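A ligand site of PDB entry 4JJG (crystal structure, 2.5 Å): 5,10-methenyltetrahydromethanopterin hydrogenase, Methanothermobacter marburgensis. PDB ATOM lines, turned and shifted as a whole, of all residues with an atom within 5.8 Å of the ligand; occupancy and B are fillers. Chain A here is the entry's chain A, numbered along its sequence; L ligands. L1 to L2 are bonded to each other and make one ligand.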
ATOM      1  N   ILE A   5      25.340 -21.110  -9.420  1.00  0.00           N
ATOM      2  CA  ILE A   5      24.061 -20.447  -9.209  1.00  0.00           C
ATOM      3  C   ILE A   5      23.377 -20.442 -10.554  1.00  0.00           C
ATOM      4  O   ILE A   5      23.959 -19.989 -11.549  1.00  0.00           O
ATOM      5  CB  ILE A   5      24.235 -18.975  -8.834  1.00  0.00           C
ATOM      6  CG1 ILE A   5      24.917 -18.832  -7.473  1.00  0.00           C
ATOM      7  CG2 ILE A   5      22.850 -18.264  -8.894  1.00  0.00           C
ATOM      8  CD1 ILE A   5      24.935 -17.410  -6.987  1.00  0.00           C
ATOM      9  N   LEU A   6      22.147 -20.940 -10.547  1.00  0.00           N
ATOM     10  CA  LEU A   6      21.389 -21.138 -11.778  1.00  0.00           C
ATOM     11  C   LEU A   6      20.098 -20.302 -11.673  1.00  0.00           C
ATOM     12  O   LEU A   6      19.127 -20.654 -10.964  1.00  0.00           O
ATOM     13  CB  LEU A   6      21.062 -22.605 -11.946  1.00  0.00           C
ATOM     14  CG  LEU A   6      21.982 -23.548 -12.748  1.00  0.00           C
ATOM     15  CD1 LEU A   6      23.480 -23.137 -12.877  1.00  0.00           C
ATOM     16  CD2 LEU A   6      21.813 -24.987 -12.252  1.00  0.00           C
ATOM     17  N   GLY A   7      20.141 -19.160 -12.364  1.00  0.00           N
ATOM     18  CA  GLY A   7      19.072 -18.179 -12.371  1.00  0.00           C
ATOM     19  C   GLY A   7      19.594 -16.969 -11.597  1.00  0.00           C
ATOM     20  O   GLY A   7      19.909 -17.083 -10.423  1.00  0.00           O
ATOM     21  N   ALA A   8      19.679 -15.813 -12.276  1.00  0.00           N
ATOM     22  CA  ALA A   8      20.101 -14.575 -11.639  1.00  0.00           C
ATOM     23  C   ALA A   8      18.932 -13.822 -11.003  1.00  0.00           C
ATOM     24  O   ALA A   8      19.146 -12.911 -10.199  1.00  0.00           O
ATOM     25  CB  ALA A   8      20.813 -13.702 -12.630  1.00  0.00           C
ATOM     26  N   GLY A   9      17.708 -14.174 -11.376  1.00  0.00           N
ATOM     27  CA  GLY A   9      16.510 -13.475 -10.927  1.00  0.00           C
ATOM     28  C   GLY A   9      16.351 -12.095 -11.520  1.00  0.00           C
ATOM     29  O   GLY A   9      17.322 -11.514 -12.058  1.00  0.00           O
ATOM     30  N   CYS A  10      15.125 -11.564 -11.438  1.00  0.00           N
ATOM     31  CA  CYS A  10      14.815 -10.222 -11.924  1.00  0.00           C
ATOM     32  C   CYS A  10      14.194  -9.429 -10.790  1.00  0.00           C
ATOM     33  O   CYS A  10      13.535  -9.997  -9.937  1.00  0.00           O
ATOM     34  CB  CYS A  10      13.828 -10.265 -13.067  1.00  0.00           C
ATOM     35  SG  CYS A  10      13.301  -8.628 -13.599  1.00  0.00           S
ATOM     36  N   TYR A  11      14.397  -8.126 -10.792  1.00  0.00           N
ATOM     37  CA  TYR A  11      13.904  -7.294  -9.692  1.00  0.00           C
ATOM     38  C   TYR A  11      12.436  -6.871  -9.808  1.00  0.00           C
ATOM     39  O   TYR A  11      11.809  -6.541  -8.796  1.00  0.00           O
ATOM     40  CB  TYR A  11      14.808  -6.061  -9.484  1.00  0.00           C
ATOM     41  CG  TYR A  11      14.612  -5.378  -8.146  1.00  0.00           C
ATOM     42  CD1 TYR A  11      15.222  -5.871  -6.998  1.00  0.00           C
ATOM     43  CD2 TYR A  11      13.804  -4.238  -8.042  1.00  0.00           C
ATOM     44  CE1 TYR A  11      15.046  -5.266  -5.779  1.00  0.00           C
ATOM     45  CE2 TYR A  11      13.616  -3.617  -6.809  1.00  0.00           C
ATOM     46  CZ  TYR A  11      14.237  -4.135  -5.680  1.00  0.00           C
ATOM     47  OH  TYR A  11      14.048  -3.532  -4.456  1.00  0.00           O
ATOM     48  N   THR A  13       9.284  -7.826  -9.896  1.00  0.00           N
ATOM     49  CA  THR A  13       8.272  -8.204  -8.912  1.00  0.00           C
ATOM     50  C   THR A  13       8.663  -7.789  -7.487  1.00  0.00           C
ATOM     51  O   THR A  13       7.788  -7.658  -6.620  1.00  0.00           O
ATOM     52  CB  THR A  13       7.961  -9.721  -8.932  1.00  0.00           C
ATOM     53  OG1 THR A  13       9.101 -10.465  -8.405  1.00  0.00           O
ATOM     54  CG2 THR A  13       7.570 -10.177 -10.387  1.00  0.00           C
ATOM     55  N   HIS A  14       9.951  -7.618  -7.213  1.00  0.00           N
ATOM     56  CA  HIS A  14      10.321  -7.005  -5.944  1.00  0.00           C
ATOM     57  C   HIS A  14       9.798  -5.579  -5.911  1.00  0.00           C
ATOM     58  O   HIS A  14       9.078  -5.232  -4.966  1.00  0.00           O
ATOM     59  CB  HIS A  14      11.849  -7.070  -5.682  1.00  0.00           C
ATOM     60  CG  HIS A  14      12.424  -8.439  -5.868  1.00  0.00           C
ATOM     61  ND1 HIS A  14      13.566  -8.866  -5.214  1.00  0.00           N
ATOM     62  CD2 HIS A  14      12.006  -9.485  -6.608  1.00  0.00           C
ATOM     63  CE1 HIS A  14      13.825 -10.110  -5.563  1.00  0.00           C
ATOM     64  NE2 HIS A  14      12.893 -10.510  -6.405  1.00  0.00           N
ATOM     65  N   SER A  17       5.931  -5.164  -5.814  1.00  0.00           N
ATOM     66  CA  SER A  17       5.302  -5.509  -4.523  1.00  0.00           C
ATOM     67  C   SER A  17       5.082  -4.287  -3.617  1.00  0.00           C
ATOM     68  O   SER A  17       4.143  -4.279  -2.808  1.00  0.00           O
ATOM     69  CB  SER A  17       6.085  -6.600  -3.784  1.00  0.00           C
ATOM     70  OG  SER A  17       7.156  -6.049  -3.028  1.00  0.00           O
ATOM     71  N   SER A  42      18.160 -11.095  -5.028  1.00  0.00           N
ATOM     72  CA  SER A  42      17.949 -12.498  -5.307  1.00  0.00           C
ATOM     73  C   SER A  42      19.233 -13.319  -5.115  1.00  0.00           C
ATOM     74  O   SER A  42      19.914 -13.263  -4.085  1.00  0.00           O
ATOM     75  CB  SER A  42      17.425 -12.675  -6.744  1.00  0.00           C
ATOM     76  OG  SER A  42      16.210 -11.990  -6.919  1.00  0.00           O
ATOM     77  N   ALA A  62      24.787 -18.756 -14.032  1.00  0.00           N
ATOM     78  CA  ALA A  62      24.326 -19.126 -15.374  1.00  0.00           C
ATOM     79  C   ALA A  62      22.889 -18.692 -15.542  1.00  0.00           C
ATOM     80  O   ALA A  62      22.046 -18.863 -14.630  1.00  0.00           O
ATOM     81  CB  ALA A  62      24.424 -20.608 -15.567  1.00  0.00           C
ATOM     82  N   ASP A  63      22.615 -18.096 -16.688  1.00  0.00           N
ATOM     83  CA  ASP A  63      21.283 -17.577 -16.985  1.00  0.00           C
ATOM     84  C   ASP A  63      21.264 -17.161 -18.452  1.00  0.00           C
ATOM     85  O   ASP A  63      22.176 -16.445 -18.911  1.00  0.00           O
ATOM     86  CB  ASP A  63      20.964 -16.405 -16.073  1.00  0.00           C
ATOM     87  CG  ASP A  63      19.474 -16.050 -16.040  1.00  0.00           C
ATOM     88  OD1 ASP A  63      18.869 -16.014 -17.138  1.00  0.00           O
ATOM     89  OD2 ASP A  63      18.929 -15.786 -14.928  1.00  0.00           O
ATOM     90  N   PRO A  64      20.255 -17.630 -19.205  1.00  0.00           N
ATOM     91  CA  PRO A  64      20.208 -17.345 -20.647  1.00  0.00           C
ATOM     92  C   PRO A  64      20.099 -15.848 -20.910  1.00  0.00           C
ATOM     93  O   PRO A  64      20.592 -15.360 -21.939  1.00  0.00           O
ATOM     94  CB  PRO A  64      18.946 -18.089 -21.124  1.00  0.00           C
ATOM     95  CG  PRO A  64      18.611 -19.069 -20.042  1.00  0.00           C
ATOM     96  CD  PRO A  64      19.103 -18.435 -18.771  1.00  0.00           C
ATOM     97  N   VAL A  65      19.496 -15.129 -19.952  1.00  0.00           N
ATOM     98  CA  VAL A  65      19.341 -13.676 -19.972  1.00  0.00           C
ATOM     99  C   VAL A  65      20.614 -12.862 -20.210  1.00  0.00           C
ATOM    100  O   VAL A  65      20.547 -11.808 -20.858  1.00  0.00           O
ATOM    101  CB  VAL A  65      18.614 -13.156 -18.710  1.00  0.00           C
ATOM    102  CG1 VAL A  65      19.589 -12.862 -17.579  1.00  0.00           C
ATOM    103  CG2 VAL A  65      17.821 -11.928 -19.054  1.00  0.00           C
ATOM    104  N   PRO A 110      11.715 -12.523 -17.776  1.00  0.00           N
ATOM    105  CA  PRO A 110      12.933 -13.295 -17.744  1.00  0.00           C
ATOM    106  C   PRO A 110      12.781 -14.644 -18.431  1.00  0.00           C
ATOM    107  O   PRO A 110      11.801 -15.344 -18.182  1.00  0.00           O
ATOM    108  CB  PRO A 110      13.159 -13.554 -16.272  1.00  0.00           C
ATOM    109  CG  PRO A 110      12.356 -12.672 -15.576  1.00  0.00           C
ATOM    110  CD  PRO A 110      11.214 -12.250 -16.431  1.00  0.00           C
ATOM    111  N   PRO A 111      13.513 -14.742 -19.531  1.00  0.00           N
ATOM    112  CA  PRO A 111      14.871 -15.295 -19.636  1.00  0.00           C
ATOM    113  C   PRO A 111      15.369 -14.308 -20.716  1.00  0.00           C
ATOM    114  O   PRO A 111      16.541 -14.298 -21.065  1.00  0.00           O
ATOM    115  CB  PRO A 111      14.685 -16.714 -20.169  1.00  0.00           C
ATOM    116  CG  PRO A 111      13.275 -16.848 -20.573  1.00  0.00           C
ATOM    117  CD  PRO A 111      12.487 -15.735 -19.921  1.00  0.00           C
ATOM    118  N   GLU A 112      14.450 -13.474 -21.191  1.00  0.00           N
ATOM    119  CA  GLU A 112      14.691 -12.480 -22.237  1.00  0.00           C
ATOM    120  C   GLU A 112      15.047 -11.106 -21.663  1.00  0.00           C
ATOM    121  O   GLU A 112      15.846 -10.383 -22.236  1.00  0.00           O
ATOM    122  CB  GLU A 112      13.470 -12.370 -23.144  1.00  0.00           C
ATOM    123  CG  GLU A 112      13.809 -11.965 -24.557  1.00  0.00           C
ATOM    124  CD  GLU A 112      14.474 -13.081 -25.367  1.00  0.00           C
ATOM    125  OE1 GLU A 112      14.049 -14.263 -25.255  1.00  0.00           O
ATOM    126  OE2 GLU A 112      15.420 -12.770 -26.128  1.00  0.00           O
ATOM    127  N   ALA A 114      15.828  -8.997 -17.740  1.00  0.00           N
ATOM    128  CA  ALA A 114      15.997  -9.021 -16.284  1.00  0.00           C
ATOM    129  C   ALA A 114      16.648  -7.704 -15.831  1.00  0.00           C
ATOM    130  O   ALA A 114      17.516  -7.154 -16.544  1.00  0.00           O
ATOM    131  CB  ALA A 114      16.806 -10.266 -15.836  1.00  0.00           C
ATOM    132  N   ASP A 131      24.045 -23.786 -18.822  1.00  0.00           N
ATOM    133  CA  ASP A 131      23.843 -24.380 -17.503  1.00  0.00           C
ATOM    134  C   ASP A 131      24.774 -25.599 -17.343  1.00  0.00           C
ATOM    135  O   ASP A 131      25.364 -25.802 -16.289  1.00  0.00           O
ATOM    136  CB  ASP A 131      22.380 -24.776 -17.270  1.00  0.00           C
ATOM    137  CG  ASP A 131      21.440 -23.554 -17.129  1.00  0.00           C
ATOM    138  OD1 ASP A 131      21.875 -22.498 -16.601  1.00  0.00           O
ATOM    139  OD2 ASP A 131      20.240 -23.673 -17.507  1.00  0.00           O
ATOM    140  N   TRP A 144      17.191 -21.275  -9.204  1.00  0.00           N
ATOM    141  CA  TRP A 144      16.301 -20.148  -8.989  1.00  0.00           C
ATOM    142  C   TRP A 144      15.516 -19.986 -10.273  1.00  0.00           C
ATOM    143  O   TRP A 144      15.782 -19.062 -11.081  1.00  0.00           O
ATOM    144  CB  TRP A 144      17.149 -18.906  -8.765  1.00  0.00           C
ATOM    145  CG  TRP A 144      16.475 -17.655  -8.263  1.00  0.00           C
ATOM    146  CD1 TRP A 144      16.084 -16.611  -9.019  1.00  0.00           C
ATOM    147  CD2 TRP A 144      16.218 -17.288  -6.902  1.00  0.00           C
ATOM    148  NE1 TRP A 144      15.546 -15.636  -8.239  1.00  0.00           N
ATOM    149  CE2 TRP A 144      15.620 -16.019  -6.921  1.00  0.00           C
ATOM    150  CE3 TRP A 144      16.461 -17.919  -5.655  1.00  0.00           C
ATOM    151  CZ2 TRP A 144      15.210 -15.345  -5.761  1.00  0.00           C
ATOM    152  CZ3 TRP A 144      16.075 -17.255  -4.476  1.00  0.00           C
ATOM    153  CH2 TRP A 144      15.431 -15.980  -4.548  1.00  0.00           C
ATOM    154  N   PHE A 145      14.585 -20.891 -10.491  1.00  0.00           N
ATOM    155  CA  PHE A 145      13.933 -21.013 -11.760  1.00  0.00           C
ATOM    156  C   PHE A 145      12.504 -20.507 -11.636  1.00  0.00           C
ATOM    157  O   PHE A 145      11.962 -20.551 -10.528  1.00  0.00           O
ATOM    158  CB  PHE A 145      13.969 -22.484 -12.151  1.00  0.00           C
ATOM    159  CG  PHE A 145      15.336 -23.012 -12.499  1.00  0.00           C
ATOM    160  CD1 PHE A 145      15.625 -24.373 -12.393  1.00  0.00           C
ATOM    161  CD2 PHE A 145      16.334 -22.148 -12.984  1.00  0.00           C
ATOM    162  CE1 PHE A 145      16.895 -24.878 -12.726  1.00  0.00           C
ATOM    163  CE2 PHE A 145      17.592 -22.650 -13.344  1.00  0.00           C
ATOM    164  CZ  PHE A 145      17.871 -24.022 -13.213  1.00  0.00           C
ATOM    165  N   PRO A 146      11.883 -20.053 -12.746  1.00  0.00           N
ATOM    166  CA  PRO A 146      10.461 -19.636 -12.740  1.00  0.00           C
ATOM    167  C   PRO A 146       9.466 -20.741 -12.310  1.00  0.00           C
ATOM    168  O   PRO A 146       9.774 -21.932 -12.404  1.00  0.00           O
ATOM    169  CB  PRO A 146      10.194 -19.221 -14.207  1.00  0.00           C
ATOM    170  CG  PRO A 146      11.261 -19.881 -15.022  1.00  0.00           C
ATOM    171  CD  PRO A 146      12.464 -20.014 -14.109  1.00  0.00           C
ATOM    172  N   LYS A 147       8.287 -20.326 -11.826  1.00  0.00           N
ATOM    173  CA  LYS A 147       7.241 -21.225 -11.352  1.00  0.00           C
ATOM    174  C   LYS A 147       6.547 -21.954 -12.505  1.00  0.00           C
ATOM    175  O   LYS A 147       6.509 -21.441 -13.610  1.00  0.00           O
ATOM    176  CB  LYS A 147       6.203 -20.457 -10.513  1.00  0.00           C
ATOM    177  CG  LYS A 147       5.394 -21.353  -9.574  1.00  0.00           C
ATOM    178  CD  LYS A 147       4.745 -20.585  -8.404  1.00  0.00           C
ATOM    179  CE  LYS A 147       3.656 -21.479  -7.795  1.00  0.00           C
ATOM    180  NZ  LYS A 147       2.560 -20.711  -7.109  1.00  0.00           N
ATOM    181  N   ILE A 154      14.090 -27.115 -18.014  1.00  0.00           N
ATOM    182  CA  ILE A 154      15.368 -26.495 -17.678  1.00  0.00           C
ATOM    183  C   ILE A 154      16.360 -27.525 -17.105  1.00  0.00           C
ATOM    184  O   ILE A 154      17.542 -27.550 -17.477  1.00  0.00           O
ATOM    185  CB  ILE A 154      15.183 -25.309 -16.703  1.00  0.00           C
ATOM    186  CG1 ILE A 154      14.392 -24.184 -17.395  1.00  0.00           C
ATOM    187  CG2 ILE A 154      16.507 -24.819 -16.240  1.00  0.00           C
ATOM    188  CD1 ILE A 154      13.725 -23.173 -16.526  1.00  0.00           C
ATOM    189  N   LYS A 157      18.032 -30.717 -19.150  1.00  0.00           N
ATOM    190  CA  LYS A 157      19.106 -30.193 -19.985  1.00  0.00           C
ATOM    191  C   LYS A 157      20.505 -30.419 -19.380  1.00  0.00           C
ATOM    192  O   LYS A 157      21.461 -30.648 -20.102  1.00  0.00           O
ATOM    193  CB  LYS A 157      18.899 -28.700 -20.244  1.00  0.00           C
ATOM    194  CG  LYS A 157      18.545 -28.365 -21.667  1.00  0.00           C
ATOM    195  CD  LYS A 157      17.050 -28.359 -21.906  1.00  0.00           C
ATOM    196  CE  LYS A 157      16.655 -27.310 -22.977  1.00  0.00           C
ATOM    197  NZ  LYS A 157      15.972 -26.135 -22.336  1.00  0.00           N
ATOM    198  N   ALA A 171      14.278 -22.845  -4.362  1.00  0.00           N
ATOM    199  CA  ALA A 171      13.780 -21.741  -3.579  1.00  0.00           C
ATOM    200  C   ALA A 171      12.233 -21.676  -3.744  1.00  0.00           C
ATOM    201  O   ALA A 171      11.557 -22.710  -3.780  1.00  0.00           O
ATOM    202  CB  ALA A 171      14.483 -20.456  -4.008  1.00  0.00           C
ATOM    203  N   CYS A 172      11.656 -20.505  -3.867  1.00  0.00           N
ATOM    204  CA  CYS A 172      10.254 -20.400  -3.555  1.00  0.00           C
ATOM    205  C   CYS A 172       9.374 -20.813  -4.732  1.00  0.00           C
ATOM    206  O   CYS A 172       8.180 -21.057  -4.587  1.00  0.00           O
ATOM    207  CB  CYS A 172       9.924 -18.974  -3.087  1.00  0.00           C
ATOM    208  SG  CYS A 172       9.586 -17.847  -4.475  1.00  0.00           S
ATOM    209  N   THR A 173       9.962 -20.895  -5.910  1.00  0.00           N
ATOM    210  CA  THR A 173       9.167 -21.181  -7.089  1.00  0.00           C
ATOM    211  C   THR A 173       8.746 -22.667  -7.248  1.00  0.00           C
ATOM    212  O   THR A 173       7.966 -22.984  -8.129  1.00  0.00           O
ATOM    213  CB  THR A 173       9.866 -20.655  -8.330  1.00  0.00           C
ATOM    214  OG1 THR A 173      11.259 -20.936  -8.243  1.00  0.00           O
ATOM    215  CG2 THR A 173       9.677 -19.139  -8.430  1.00  0.00           C
ATOM    216  N   HIS A 203      16.025 -21.441   0.721  1.00  0.00           N
ATOM    217  CA  HIS A 203      14.849 -20.637   0.450  1.00  0.00           C
ATOM    218  C   HIS A 203      14.962 -19.417   1.393  1.00  0.00           C
ATOM    219  O   HIS A 203      15.109 -19.584   2.613  1.00  0.00           O
ATOM    220  CB  HIS A 203      13.651 -21.519   0.773  1.00  0.00           C
ATOM    221  CG  HIS A 203      12.311 -20.948   0.437  1.00  0.00           C
ATOM    222  ND1 HIS A 203      12.021 -19.605   0.487  1.00  0.00           N
ATOM    223  CD2 HIS A 203      11.149 -21.559   0.084  1.00  0.00           C
ATOM    224  CE1 HIS A 203      10.749 -19.404   0.171  1.00  0.00           C
ATOM    225  NE2 HIS A 203      10.193 -20.582  -0.076  1.00  0.00           N
ATOM    226  N   PRO A 204      14.919 -18.222   0.840  1.00  0.00           N
ATOM    227  CA  PRO A 204      15.118 -17.031   1.666  1.00  0.00           C
ATOM    228  C   PRO A 204      13.875 -16.656   2.481  1.00  0.00           C
ATOM    229  O   PRO A 204      13.970 -15.881   3.456  1.00  0.00           O
ATOM    230  CB  PRO A 204      15.464 -15.924   0.644  1.00  0.00           C
ATOM    231  CG  PRO A 204      14.889 -16.387  -0.647  1.00  0.00           C
ATOM    232  CD  PRO A 204      15.022 -17.931  -0.594  1.00  0.00           C
ATOM    233  N   GLY A 205      12.730 -17.188   2.100  1.00  0.00           N
ATOM    234  CA  GLY A 205      11.531 -16.906   2.846  1.00  0.00           C
ATOM    235  C   GLY A 205      11.070 -15.445   2.746  1.00  0.00           C
ATOM    236  O   GLY A 205      10.352 -14.964   3.620  1.00  0.00           O
ATOM    237  N   ALA A 206      11.477 -14.767   1.657  1.00  0.00           N
ATOM    238  CA  ALA A 206      11.401 -13.310   1.497  1.00  0.00           C
ATOM    239  C   ALA A 206      12.475 -12.924   0.461  1.00  0.00           C
ATOM    240  O   ALA A 206      13.381 -13.714   0.211  1.00  0.00           O
ATOM    241  CB  ALA A 206      11.680 -12.570   2.840  1.00  0.00           C
ATOM    242  N   VAL A 207      12.428 -11.736  -0.120  1.00  0.00           N
ATOM    243  CA  VAL A 207      13.523 -11.350  -1.019  1.00  0.00           C
ATOM    244  C   VAL A 207      14.786 -11.259  -0.193  1.00  0.00           C
ATOM    245  O   VAL A 207      14.822 -10.581   0.855  1.00  0.00           O
ATOM    246  CB  VAL A 207      13.225 -10.067  -1.853  1.00  0.00           C
ATOM    247  CG1 VAL A 207      11.868 -10.191  -2.546  1.00  0.00           C
ATOM    248  CG2 VAL A 207      13.320  -8.760  -1.021  1.00  0.00           C
ATOM    249  N   PRO A 208      15.816 -11.978  -0.640  1.00  0.00           N
ATOM    250  CA  PRO A 208      17.058 -12.112   0.150  1.00  0.00           C
ATOM    251  C   PRO A 208      17.753 -10.760   0.426  1.00  0.00           C
ATOM    252  O   PRO A 208      18.390 -10.607   1.468  1.00  0.00           O
ATOM    253  CB  PRO A 208      17.951 -13.016  -0.705  1.00  0.00           C
ATOM    254  CG  PRO A 208      17.339 -12.983  -2.053  1.00  0.00           C
ATOM    255  CD  PRO A 208      15.878 -12.726  -1.911  1.00  0.00           C
ATOM    256  N   GLU A 209      17.606  -9.784  -0.466  1.00  0.00           N
ATOM    257  CA  GLU A 209      18.311  -8.513  -0.279  1.00  0.00           C
ATOM    258  C   GLU A 209      17.736  -7.726   0.907  1.00  0.00           C
ATOM    259  O   GLU A 209      18.382  -6.803   1.421  1.00  0.00           O
ATOM    260  CB  GLU A 209      18.314  -7.665  -1.560  1.00  0.00           C
ATOM    261  CG  GLU A 209      16.932  -7.194  -2.005  1.00  0.00           C
ATOM    262  CD  GLU A 209      16.149  -8.218  -2.867  1.00  0.00           C
ATOM    263  OE1 GLU A 209      16.561  -9.392  -3.038  1.00  0.00           O
ATOM    264  OE2 GLU A 209      15.095  -7.812  -3.375  1.00  0.00           O
HETATM  265  O1  LIG L   1      10.060 -13.899  -6.303  1.00  0.00           O
HETATM  266 FE1  LIG L   1      11.066 -15.666  -4.217  1.00  0.00          FE
HETATM  267  C1  LIG L   1      12.420 -14.421  -4.092  1.00  0.00           C
HETATM  268  O2  LIG L   1      13.299 -13.623  -3.990  1.00  0.00           O
HETATM  269  C2  LIG L   1      10.782 -15.683  -2.389  1.00  0.00           C
HETATM  270  O3  LIG L   1      10.615 -15.701  -1.192  1.00  0.00           O
HETATM  271  C3  LIG L   1      12.270 -17.181  -4.654  1.00  0.00           C
HETATM  272  O4  LIG L   1      12.582 -17.796  -3.406  1.00  0.00           O
HETATM  273  C4  LIG L   1      12.726 -17.660  -5.979  1.00  0.00           C
HETATM  274  C5  LIG L   1      12.082 -16.634  -6.863  1.00  0.00           C
HETATM  275  N1  LIG L   1      11.366 -15.686  -6.253  1.00  0.00           N
HETATM  276  C6  LIG L   1      12.266 -16.689  -8.237  1.00  0.00           C
HETATM  277  C7  LIG L   1      13.087 -17.778  -8.875  1.00  0.00           C
HETATM  278  C8  LIG L   1      11.659 -15.727  -9.015  1.00  0.00           C
HETATM  279  C9  LIG L   1      10.864 -14.733  -8.395  1.00  0.00           C
HETATM  280  C10 LIG L   1      10.157 -13.642  -9.172  1.00  0.00           C
HETATM  281  C11 LIG L   1      10.773 -14.796  -6.998  1.00  0.00           C
HETATM  282  O5  LIG L   1      11.827 -15.779 -10.371  1.00  0.00           O
HETATM  283  P1  LIG L   1      12.761 -14.789 -11.228  1.00  0.00           P
HETATM  284  O6  LIG L   1      12.064 -14.432 -12.542  1.00  0.00           O
HETATM  285  O7  LIG L   1      13.293 -13.682 -10.332  1.00  0.00           O
HETATM  286  O8  LIG L   1      14.001 -15.774 -11.455  1.00  0.00           O
HETATM  287  C12 LIG L   1      13.935 -16.831 -12.423  1.00  0.00           C
HETATM  288  C13 LIG L   1      15.228 -16.786 -13.221  1.00  0.00           C
HETATM  289  O9  LIG L   1      15.376 -17.990 -13.963  1.00  0.00           O
HETATM  290  C14 LIG L   1      16.097 -17.677 -15.158  1.00  0.00           C
HETATM  291  C15 LIG L   1      15.491 -16.361 -15.583  1.00  0.00           C
HETATM  292  O10 LIG L   1      16.445 -15.688 -16.405  1.00  0.00           O
HETATM  293  C16 LIG L   1      15.276 -15.682 -14.255  1.00  0.00           C
HETATM  294  O11 LIG L   1      16.433 -14.923 -13.910  1.00  0.00           O
HETATM  295  N2  LIG L   1      16.013 -18.789 -16.147  1.00  0.00           N
HETATM  296  C17 LIG L   1      16.963 -19.710 -16.293  1.00  0.00           C
HETATM  297  N3  LIG L   1      18.171 -19.909 -15.711  1.00  0.00           N
HETATM  298  C18 LIG L   1      18.986 -20.908 -16.067  1.00  0.00           C
HETATM  299  N4  LIG L   1      20.185 -21.032 -15.432  1.00  0.00           N
HETATM  300  N5  LIG L   1      18.605 -21.794 -17.037  1.00  0.00           N
HETATM  301  C19 LIG L   1      17.396 -21.645 -17.653  1.00  0.00           C
HETATM  302  O12 LIG L   1      16.981 -22.522 -18.610  1.00  0.00           O
HETATM  303  C20 LIG L   1      16.552 -20.579 -17.292  1.00  0.00           C
HETATM  304  N6  LIG L   1      15.339 -20.162 -17.700  1.00  0.00           N
HETATM  305  C21 LIG L   1      15.013 -19.063 -16.986  1.00  0.00           C
HETATM  306  O1  LG2 L   2       7.407 -11.217  -6.458  1.00  0.00           O
HETATM  307  S1  LG2 L   2       7.328 -12.006  -5.265  1.00  0.00           S
HETATM  308  O2  LG2 L   2       6.818 -11.193  -4.192  1.00  0.00           O
HETATM  309  C1  LG2 L   2       6.310 -13.336  -5.459  1.00  0.00           C
HETATM  310  C2  LG2 L   2       6.448 -14.225  -6.701  1.00  0.00           C
HETATM  311  C3  LG2 L   2       6.793 -15.585  -6.536  1.00  0.00           C
HETATM  312  C4  LG2 L   2       6.925 -16.442  -7.637  1.00  0.00           C
HETATM  313  C5  LG2 L   2       6.696 -15.938  -8.922  1.00  0.00           C
HETATM  314  C6  LG2 L   2       6.846 -16.850 -10.121  1.00  0.00           C
HETATM  315  C7  LG2 L   2       6.336 -14.598  -9.090  1.00  0.00           C
HETATM  316  C8  LG2 L   2       6.204 -13.742  -7.989  1.00  0.00           C
HETATM  317  C9  LG2 L   2       8.802 -12.420  -4.862  1.00  0.00           C
HETATM  318  N1  LG2 L   2       9.413 -13.507  -4.219  1.00  0.00           N
HETATM  319  C10 LG2 L   2      10.085 -14.234  -4.962  1.00  0.00           C
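N of Gly 205 lies within hydrogen-bond range of ND1 of His 203, at 3.0 Å. N of Ala 8 lies within hydrogen-bond range of OD2 of Asp 63 (2.8 Å). OG of Ser 17 is in hydrogen-bond range of O of His 14 (2.8 Å). OD1 of Asp 63 is in hydrogen-bond range of N of Val 65. The backbone carbonyl oxygen (O) of Ala 62 lies within hydrogen-bond range of the backbone NH (N) of Gly 7 (3.0 Å). The backbone carbonyl oxygen of Phe 145 lies within hydrogen-bond range of the side-chain hydroxyl of Thr 173 (2.4 Å). The backbone NH of Ala 62 is in hydrogen-bond range of the backbone carbonyl oxygen of Ile 5. The backbone NH of Val 65 sits close to the backbone carbonyl oxygen of Pro 111 (3.3 Å).
The side-chain hydroxyl (OG1) of Thr 13 lies within hydrogen-bond range of an oxygen (O1) of LG2 L2 (2.7 Å). The backbone NH (N) of Gly 9 sits at hydrogen-bond distance from an oxygen (O11) of LIG L1 (2.9 Å). An iron atom (FE1) of LIG L1 is bound by the side-chain sulfur of Cys 172. The backbone carbonyl oxygen (O) of Ala 62 lies within hydrogen-bond range of a nitrogen (N4) of LIG L1, 3.0 Å away. OD1 of Asp 63 lies within hydrogen-bond range of O10 of LIG L1, 2.6 Å away. A nitrogen (N4) of LIG L1 lies within hydrogen-bond range of the side-chain carboxylate of Asp 131 (2.5 Å). The backbone NH (N) of Ala 206 lies within hydrogen-bond range of an oxygen (O3) of LIG L1 (3.1 Å). N of Cys 10 sits at hydrogen-bond distance from O7 of LIG L1 (3.0 Å). The backbone NH of Cys 172 lies within hydrogen-bond range of an oxygen (O4) of LIG L1.
The backbone carbonyl oxygen (O) of Trp 144 sits close to an oxygen (O9) of LIG L1 (3.1 Å). Merely in contact with the ligand: Ile 154, Ala 171, Phe 145, Pro 208, Pro 64, Pro 110, Pro 146, Thr 173, Gly 7, Pro 111, Lys 147, Pro 204, Ala 8, Val 207, Leu 6, His 14, His 203 and Gly 205. Of the 36 residues printed, 27 come within 4 Å of the ligand.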
